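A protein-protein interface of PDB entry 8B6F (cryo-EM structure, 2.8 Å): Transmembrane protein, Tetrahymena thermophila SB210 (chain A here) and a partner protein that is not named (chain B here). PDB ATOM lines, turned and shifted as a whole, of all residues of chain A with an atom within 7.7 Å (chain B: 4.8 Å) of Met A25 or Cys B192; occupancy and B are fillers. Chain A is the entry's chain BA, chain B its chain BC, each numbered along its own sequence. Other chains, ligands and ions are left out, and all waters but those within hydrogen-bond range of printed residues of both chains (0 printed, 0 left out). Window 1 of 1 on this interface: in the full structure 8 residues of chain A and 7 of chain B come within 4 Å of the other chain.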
ATOM      1  N   VAL A  16     -26.912  12.683   4.488  1.00  0.00           N
ATOM      2  CA  VAL A  16     -25.799  13.622   4.553  1.00  0.00           C
ATOM      3  C   VAL A  16     -24.612  13.046   3.799  1.00  0.00           C
ATOM      4  O   VAL A  16     -24.261  11.873   3.965  1.00  0.00           O
ATOM      5  CB  VAL A  16     -25.448  13.933   6.020  1.00  0.00           C
ATOM      6  CG1 VAL A  16     -25.062  12.663   6.769  1.00  0.00           C
ATOM      7  CG2 VAL A  16     -24.332  14.966   6.095  1.00  0.00           C
ATOM      8  N   GLN A  18     -21.042  12.002   2.847  1.00  0.00           N
ATOM      9  CA  GLN A  18     -19.879  11.667   3.662  1.00  0.00           C
ATOM     10  C   GLN A  18     -18.713  12.607   3.384  1.00  0.00           C
ATOM     11  O   GLN A  18     -18.030  13.051   4.314  1.00  0.00           O
ATOM     12  CB  GLN A  18     -19.467  10.216   3.409  1.00  0.00           C
ATOM     13  CG  GLN A  18     -20.500   9.196   3.861  1.00  0.00           C
ATOM     14  CD  GLN A  18     -20.713   9.204   5.362  1.00  0.00           C
ATOM     15  OE1 GLN A  18     -19.888   9.720   6.115  1.00  0.00           O
ATOM     16  NE2 GLN A  18     -21.827   8.632   5.803  1.00  0.00           N
ATOM     17  N   HIS A  19     -18.474  12.931   2.112  1.00  0.00           N
ATOM     18  CA  HIS A  19     -17.352  13.801   1.777  1.00  0.00           C
ATOM     19  C   HIS A  19     -17.544  15.198   2.349  1.00  0.00           C
ATOM     20  O   HIS A  19     -16.603  15.790   2.891  1.00  0.00           O
ATOM     21  CB  HIS A  19     -17.171  13.866   0.261  1.00  0.00           C
ATOM     22  CG  HIS A  19     -16.784  12.557  -0.350  1.00  0.00           C
ATOM     23  ND1 HIS A  19     -17.712  11.603  -0.713  1.00  0.00           N
ATOM     24  CD2 HIS A  19     -15.572  12.034  -0.647  1.00  0.00           C
ATOM     25  CE1 HIS A  19     -17.087  10.553  -1.215  1.00  0.00           C
ATOM     26  NE2 HIS A  19     -15.787  10.789  -1.186  1.00  0.00           N
ATOM     27  N   GLU A  20     -18.756  15.744   2.240  1.00  0.00           N
ATOM     28  CA  GLU A  20     -19.012  17.064   2.806  1.00  0.00           C
ATOM     29  C   GLU A  20     -18.876  17.043   4.322  1.00  0.00           C
ATOM     30  O   GLU A  20     -18.296  17.959   4.914  1.00  0.00           O
ATOM     31  CB  GLU A  20     -20.402  17.548   2.397  1.00  0.00           C
ATOM     32  CG  GLU A  20     -20.577  17.747   0.902  1.00  0.00           C
ATOM     33  CD  GLU A  20     -19.695  18.853   0.355  1.00  0.00           C
ATOM     34  OE1 GLU A  20     -19.067  19.570   1.161  1.00  0.00           O
ATOM     35  OE2 GLU A  20     -19.633  19.009  -0.883  1.00  0.00           O
ATOM     36  N   LEU A  21     -19.407  16.003   4.969  1.00  0.00           N
ATOM     37  CA  LEU A  21     -19.277  15.900   6.419  1.00  0.00           C
ATOM     38  C   LEU A  21     -17.812  15.816   6.829  1.00  0.00           C
ATOM     39  O   LEU A  21     -17.387  16.476   7.784  1.00  0.00           O
ATOM     40  CB  LEU A  21     -20.047  14.684   6.931  1.00  0.00           C
ATOM     41  CG  LEU A  21     -19.987  14.438   8.442  1.00  0.00           C
ATOM     42  CD1 LEU A  21     -20.556  15.620   9.212  1.00  0.00           C
ATOM     43  CD2 LEU A  21     -20.727  13.160   8.802  1.00  0.00           C
ATOM     44  N   LYS A  22     -17.023  15.018   6.108  1.00  0.00           N
ATOM     45  CA  LYS A  22     -15.605  14.897   6.427  1.00  0.00           C
ATOM     46  C   LYS A  22     -14.873  16.213   6.200  1.00  0.00           C
ATOM     47  O   LYS A  22     -13.994  16.581   6.986  1.00  0.00           O
ATOM     48  CB  LYS A  22     -14.974  13.779   5.600  1.00  0.00           C
ATOM     49  CG  LYS A  22     -15.392  12.388   6.039  1.00  0.00           C
ATOM     50  CD  LYS A  22     -14.658  11.313   5.252  1.00  0.00           C
ATOM     51  CE  LYS A  22     -15.100   9.922   5.672  1.00  0.00           C
ATOM     52  NZ  LYS A  22     -14.898   9.685   7.127  1.00  0.00           N
ATOM     53  N   ALA A  23     -15.224  16.941   5.140  1.00  0.00           N
ATOM     54  CA  ALA A  23     -14.593  18.235   4.908  1.00  0.00           C
ATOM     55  C   ALA A  23     -14.900  19.204   6.042  1.00  0.00           C
ATOM     56  O   ALA A  23     -14.009  19.922   6.511  1.00  0.00           O
ATOM     57  CB  ALA A  23     -15.053  18.811   3.569  1.00  0.00           C
ATOM     58  N   GLU A  24     -16.153  19.244   6.498  1.00  0.00           N
ATOM     59  CA  GLU A  24     -16.499  20.117   7.615  1.00  0.00           C
ATOM     60  C   GLU A  24     -15.750  19.718   8.877  1.00  0.00           C
ATOM     61  O   GLU A  24     -15.242  20.578   9.606  1.00  0.00           O
ATOM     62  CB  GLU A  24     -18.005  20.082   7.864  1.00  0.00           C
ATOM     63  CG  GLU A  24     -18.811  20.863   6.853  1.00  0.00           C
ATOM     64  CD  GLU A  24     -18.557  22.355   6.933  1.00  0.00           C
ATOM     65  OE1 GLU A  24     -17.927  22.797   7.916  1.00  0.00           O
ATOM     66  OE2 GLU A  24     -18.986  23.083   6.014  1.00  0.00           O
ATOM     67  N   MET A  25     -15.677  18.417   9.155  1.00  0.00           N
ATOM     68  CA  MET A  25     -14.975  17.955  10.346  1.00  0.00           C
ATOM     69  C   MET A  25     -13.484  18.261  10.256  1.00  0.00           C
ATOM     70  O   MET A  25     -12.854  18.598  11.266  1.00  0.00           O
ATOM     71  CB  MET A  25     -15.217  16.461  10.556  1.00  0.00           C
ATOM     72  CG  MET A  25     -16.652  16.104  10.917  1.00  0.00           C
ATOM     73  SD  MET A  25     -16.877  14.356  11.296  1.00  0.00           S
ATOM     74  CE  MET A  25     -15.972  14.226  12.836  1.00  0.00           C
ATOM     75  N   ILE A  26     -12.900  18.155   9.059  1.00  0.00           N
ATOM     76  CA  ILE A  26     -11.496  18.527   8.890  1.00  0.00           C
ATOM     77  C   ILE A  26     -11.308  20.007   9.195  1.00  0.00           C
ATOM     78  O   ILE A  26     -10.404  20.396   9.945  1.00  0.00           O
ATOM     79  CB  ILE A  26     -11.009  18.189   7.467  1.00  0.00           C
ATOM     80  CG1 ILE A  26     -10.915  16.675   7.266  1.00  0.00           C
ATOM     81  CG2 ILE A  26      -9.650  18.833   7.189  1.00  0.00           C
ATOM     82  CD1 ILE A  26     -10.701  16.247   5.833  1.00  0.00           C
ATOM     83  N   LYS A  27     -12.154  20.856   8.609  1.00  0.00           N
ATOM     84  CA  LYS A  27     -12.058  22.287   8.873  1.00  0.00           C
ATOM     85  C   LYS A  27     -12.175  22.580  10.364  1.00  0.00           C
ATOM     86  O   LYS A  27     -11.510  23.484  10.881  1.00  0.00           O
ATOM     87  CB  LYS A  27     -13.144  23.030   8.095  1.00  0.00           C
ATOM     88  CG  LYS A  27     -12.996  22.939   6.581  1.00  0.00           C
ATOM     89  CD  LYS A  27     -14.244  23.449   5.871  1.00  0.00           C
ATOM     90  CE  LYS A  27     -14.139  23.257   4.365  1.00  0.00           C
ATOM     91  NZ  LYS A  27     -15.372  23.705   3.657  1.00  0.00           N
ATOM     92  N   GLU A  28     -13.019  21.827  11.070  1.00  0.00           N
ATOM     93  CA  GLU A  28     -13.240  22.092  12.487  1.00  0.00           C
ATOM     94  C   GLU A  28     -12.095  21.582  13.355  1.00  0.00           C
ATOM     95  O   GLU A  28     -11.731  22.230  14.343  1.00  0.00           O
ATOM     96  CB  GLU A  28     -14.559  21.460  12.932  1.00  0.00           C
ATOM     97  CG  GLU A  28     -14.989  21.843  14.339  1.00  0.00           C
ATOM     98  CD  GLU A  28     -15.269  23.328  14.480  1.00  0.00           C
ATOM     99  OE1 GLU A  28     -15.363  24.020  13.445  1.00  0.00           O
ATOM    100  OE2 GLU A  28     -15.393  23.804  15.628  1.00  0.00           O
ATOM    101  N   LEU A  29     -11.514  20.432  13.011  1.00  0.00           N
ATOM    102  CA  LEU A  29     -10.622  19.715  13.914  1.00  0.00           C
ATOM    103  C   LEU A  29      -9.179  19.665  13.434  1.00  0.00           C
ATOM    104  O   LEU A  29      -8.363  18.969  14.045  1.00  0.00           O
ATOM    105  CB  LEU A  29     -11.136  18.292  14.135  1.00  0.00           C
ATOM    106  CG  LEU A  29     -12.533  18.172  14.743  1.00  0.00           C
ATOM    107  CD1 LEU A  29     -12.977  16.722  14.769  1.00  0.00           C
ATOM    108  CD2 LEU A  29     -12.568  18.767  16.141  1.00  0.00           C
ATOM    109  N   SER A  30      -8.835  20.373  12.357  1.00  0.00           N
ATOM    110  CA  SER A  30      -7.445  20.374  11.918  1.00  0.00           C
ATOM    111  C   SER A  30      -6.521  20.941  12.989  1.00  0.00           C
ATOM    112  O   SER A  30      -5.367  20.513  13.104  1.00  0.00           O
ATOM    113  CB  SER A  30      -7.304  21.172  10.621  1.00  0.00           C
ATOM    114  OG  SER A  30      -5.956  21.190  10.179  1.00  0.00           O
ATOM    115  N   HIS A  31      -7.005  21.907  13.771  1.00  0.00           N
ATOM    116  CA  HIS A  31      -6.155  22.579  14.749  1.00  0.00           C
ATOM    117  C   HIS A  31      -5.568  21.619  15.774  1.00  0.00           C
ATOM    118  O   HIS A  31      -4.546  21.940  16.390  1.00  0.00           O
ATOM    119  CB  HIS A  31      -6.945  23.673  15.469  1.00  0.00           C
ATOM    120  CG  HIS A  31      -7.568  24.676  14.548  1.00  0.00           C
ATOM    121  ND1 HIS A  31      -8.388  25.689  14.998  1.00  0.00           N
ATOM    122  CD2 HIS A  31      -7.491  24.825  13.205  1.00  0.00           C
ATOM    123  CE1 HIS A  31      -8.790  26.416  13.970  1.00  0.00           C
ATOM    124  NE2 HIS A  31      -8.261  25.913  12.871  1.00  0.00           N
ATOM    125  N   TYR A  33      -5.126  17.776  15.383  1.00  0.00           N
ATOM    126  CA  TYR A  33      -4.329  16.669  14.868  1.00  0.00           C
ATOM    127  C   TYR A  33      -3.397  17.072  13.735  1.00  0.00           C
ATOM    128  O   TYR A  33      -2.696  16.208  13.200  1.00  0.00           O
ATOM    129  CB  TYR A  33      -5.246  15.539  14.391  1.00  0.00           C
ATOM    130  CG  TYR A  33      -5.958  15.823  13.088  1.00  0.00           C
ATOM    131  CD1 TYR A  33      -7.188  16.464  13.072  1.00  0.00           C
ATOM    132  CD2 TYR A  33      -5.405  15.440  11.875  1.00  0.00           C
ATOM    133  CE1 TYR A  33      -7.844  16.721  11.883  1.00  0.00           C
ATOM    134  CE2 TYR A  33      -6.051  15.691  10.682  1.00  0.00           C
ATOM    135  CZ  TYR A  33      -7.270  16.331  10.692  1.00  0.00           C
ATOM    136  OH  TYR A  33      -7.915  16.581   9.505  1.00  0.00           O
ATOM    137  N   VAL B 188     -19.232  17.099  18.094  1.00  0.00           N
ATOM    138  CA  VAL B 188     -18.675  17.762  16.918  1.00  0.00           C
ATOM    139  C   VAL B 188     -19.218  17.128  15.644  1.00  0.00           C
ATOM    140  O   VAL B 188     -19.581  17.829  14.692  1.00  0.00           O
ATOM    141  CB  VAL B 188     -17.136  17.723  16.963  1.00  0.00           C
ATOM    142  CG1 VAL B 188     -16.538  18.138  15.623  1.00  0.00           C
ATOM    143  CG2 VAL B 188     -16.619  18.621  18.071  1.00  0.00           C
ATOM    144  N   GLU B 189     -19.278  15.797  15.602  1.00  0.00           N
ATOM    145  CA  GLU B 189     -19.822  15.129  14.426  1.00  0.00           C
ATOM    146  C   GLU B 189     -21.272  15.530  14.193  1.00  0.00           C
ATOM    147  O   GLU B 189     -21.669  15.822  13.060  1.00  0.00           O
ATOM    148  CB  GLU B 189     -19.706  13.613  14.585  1.00  0.00           C
ATOM    149  CG  GLU B 189     -20.193  12.825  13.378  1.00  0.00           C
ATOM    150  CD  GLU B 189     -20.175  11.330  13.615  1.00  0.00           C
ATOM    151  OE1 GLU B 189     -19.716  10.904  14.696  1.00  0.00           O
ATOM    152  OE2 GLU B 189     -20.623  10.578  12.724  1.00  0.00           O
ATOM    153  N   LYS B 190     -22.080  15.553  15.256  1.00  0.00           N
ATOM    154  CA  LYS B 190     -23.482  15.925  15.107  1.00  0.00           C
ATOM    155  C   LYS B 190     -23.622  17.366  14.636  1.00  0.00           C
ATOM    156  O   LYS B 190     -24.448  17.666  13.766  1.00  0.00           O
ATOM    157  CB  LYS B 190     -24.227  15.720  16.427  1.00  0.00           C
ATOM    158  CG  LYS B 190     -24.300  14.270  16.887  1.00  0.00           C
ATOM    159  CD  LYS B 190     -25.085  13.406  15.912  1.00  0.00           C
ATOM    160  CE  LYS B 190     -25.238  11.985  16.433  1.00  0.00           C
ATOM    161  NZ  LYS B 190     -23.924  11.328  16.687  1.00  0.00           N
ATOM    162  N   GLU B 191     -22.822  18.276  15.195  1.00  0.00           N
ATOM    163  CA  GLU B 191     -22.897  19.673  14.779  1.00  0.00           C
ATOM    164  C   GLU B 191     -22.512  19.833  13.315  1.00  0.00           C
ATOM    165  O   GLU B 191     -23.159  20.582  12.574  1.00  0.00           O
ATOM    166  CB  GLU B 191     -21.998  20.535  15.666  1.00  0.00           C
ATOM    167  CG  GLU B 191     -22.506  20.687  17.092  1.00  0.00           C
ATOM    168  CD  GLU B 191     -21.570  21.506  17.961  1.00  0.00           C
ATOM    169  OE1 GLU B 191     -20.578  22.045  17.426  1.00  0.00           O
ATOM    170  OE2 GLU B 191     -21.824  21.609  19.180  1.00  0.00           O
ATOM    171  N   CYS B 192     -21.460  19.140  12.878  1.00  0.00           N
ATOM    172  CA  CYS B 192     -21.071  19.207  11.474  1.00  0.00           C
ATOM    173  C   CYS B 192     -22.169  18.657  10.575  1.00  0.00           C
ATOM    174  O   CYS B 192     -22.467  19.232   9.522  1.00  0.00           O
ATOM    175  CB  CYS B 192     -19.761  18.453  11.258  1.00  0.00           C
ATOM    176  SG  CYS B 192     -18.347  19.279  12.014  1.00  0.00           S
ATOM    177  N   GLU B 193     -22.783  17.542  10.972  1.00  0.00           N
ATOM    178  CA  GLU B 193     -23.865  16.974  10.175  1.00  0.00           C
ATOM    179  C   GLU B 193     -25.028  17.949  10.063  1.00  0.00           C
ATOM    180  O   GLU B 193     -25.592  18.133   8.979  1.00  0.00           O
ATOM    181  CB  GLU B 193     -24.328  15.655  10.791  1.00  0.00           C
ATOM    182  CG  GLU B 193     -25.452  14.976  10.023  1.00  0.00           C
ATOM    183  CD  GLU B 193     -25.871  13.663  10.652  1.00  0.00           C
ATOM    184  OE1 GLU B 193     -25.355  13.336  11.742  1.00  0.00           O
ATOM    185  OE2 GLU B 193     -26.715  12.959  10.060  1.00  0.00           O
ATOM    186  N   GLN B 194     -25.404  18.583  11.175  1.00  0.00           N
ATOM    187  CA  GLN B 194     -26.511  19.532  11.143  1.00  0.00           C
ATOM    188  C   GLN B 194     -26.172  20.747  10.289  1.00  0.00           C
ATOM    189  O   GLN B 194     -27.025  21.246   9.546  1.00  0.00           O
ATOM    190  CB  GLN B 194     -26.880  19.958  12.564  1.00  0.00           C
ATOM    191  CG  GLN B 194     -27.420  18.825  13.428  1.00  0.00           C
ATOM    192  CD  GLN B 194     -28.688  18.208  12.870  1.00  0.00           C
ATOM    193  OE1 GLN B 194     -29.307  18.751  11.956  1.00  0.00           O
ATOM    194  NE2 GLN B 194     -29.079  17.062  13.417  1.00  0.00           N
ATOM    195  N   ARG B 195     -24.932  21.236  10.373  1.00  0.00           N
ATOM    196  CA  ARG B 195     -24.536  22.365   9.535  1.00  0.00           C
ATOM    197  C   ARG B 195     -24.604  21.999   8.057  1.00  0.00           C
ATOM    198  O   ARG B 195     -25.047  22.805   7.231  1.00  0.00           O
ATOM    199  CB  ARG B 195     -23.130  22.834   9.906  1.00  0.00           C
ATOM    200  CG  ARG B 195     -23.052  23.571  11.237  1.00  0.00           C
ATOM    201  CD  ARG B 195     -21.873  24.536  11.270  1.00  0.00           C
ATOM    202  NE  ARG B 195     -20.597  23.861  11.054  1.00  0.00           N
ATOM    203  CZ  ARG B 195     -19.841  23.350  12.016  1.00  0.00           C
ATOM    204  NH1 ARG B 195     -20.203  23.409  13.287  1.00  0.00           N
ATOM    205  NH2 ARG B 195     -18.690  22.766  11.694  1.00  0.00           N
ATOM    206  N   ILE B 196     -24.165  20.790   7.701  1.00  0.00           N
ATOM    207  CA  ILE B 196     -24.260  20.352   6.312  1.00  0.00           C
ATOM    208  C   ILE B 196     -25.717  20.280   5.876  1.00  0.00           C
ATOM    209  O   ILE B 196     -26.076  20.730   4.780  1.00  0.00           O
ATOM    210  CB  ILE B 196     -23.544  19.000   6.126  1.00  0.00           C
ATOM    211  CG1 ILE B 196     -22.021  19.173   6.140  1.00  0.00           C
ATOM    212  CG2 ILE B 196     -23.992  18.309   4.835  1.00  0.00           C
ATOM    213  CD1 ILE B 196     -21.476  20.009   4.993  1.00  0.00           C
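OE1 of Glu A24 is in salt-bridge range of NH2 of Arg B195 (3.9 Å).
The side-chain carboxylate (OE1) of Glu A28 lies within salt-bridge range of the guanidinium group (NH2) of Arg B195, at 3.96 Å.
Hydrophobic or aromatic side chains of chain B within 4 Å of the printed part of chain A: Val B188 and Ile B196.
Of the 16 printed residues of chain A, 7 touch a printed residue of chain B.
Hydrophobic or aromatic side chains of chain A within 4 Å of the printed part of chain B: Val A16, Leu A21, Met A25 and Leu A29.
Printed residues of chain B within 4 Å of Met A25: Cys B192 (3.8 Å).
Of the printed residues of chain A, Glu B193 touches Val A16 and Leu A21.
Of the printed residues of chain B, Glu A24 touches Arg B195 and Ile B196.
Lys A22 touches none of the printed residues of chain B.
Ser A30 touches none of the printed residues of chain B.
The nearest residue of chain B that does not touch Met A25 is Glu B189 (4.2 Å).
Among the printed residues, merely in contact across the chains: Val A16 with Glu B193 (3.7 Å), Val A16 with Ile B196 (3.6 Å), Glu A20 with Ile B196 (3.7 Å), Leu A21 with Cys B192 (3.6 Å), Leu A21 with Glu B193 (3.4 Å), Glu A24 with Ile B196 (3.4 Å), Met A25 with Cys B192 (3.8 Å) and Leu A29 with Val B188 (3.9 Å).
O of Val B188 sits at hydrogen-bond distance from SG of Cys B192, 3.3 Å away.
The side-chain sulfur (SG) of Cys B192 sits at hydrogen-bond distance from the guanidinium group (NH2) of Arg B195, at 3.5 Å.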
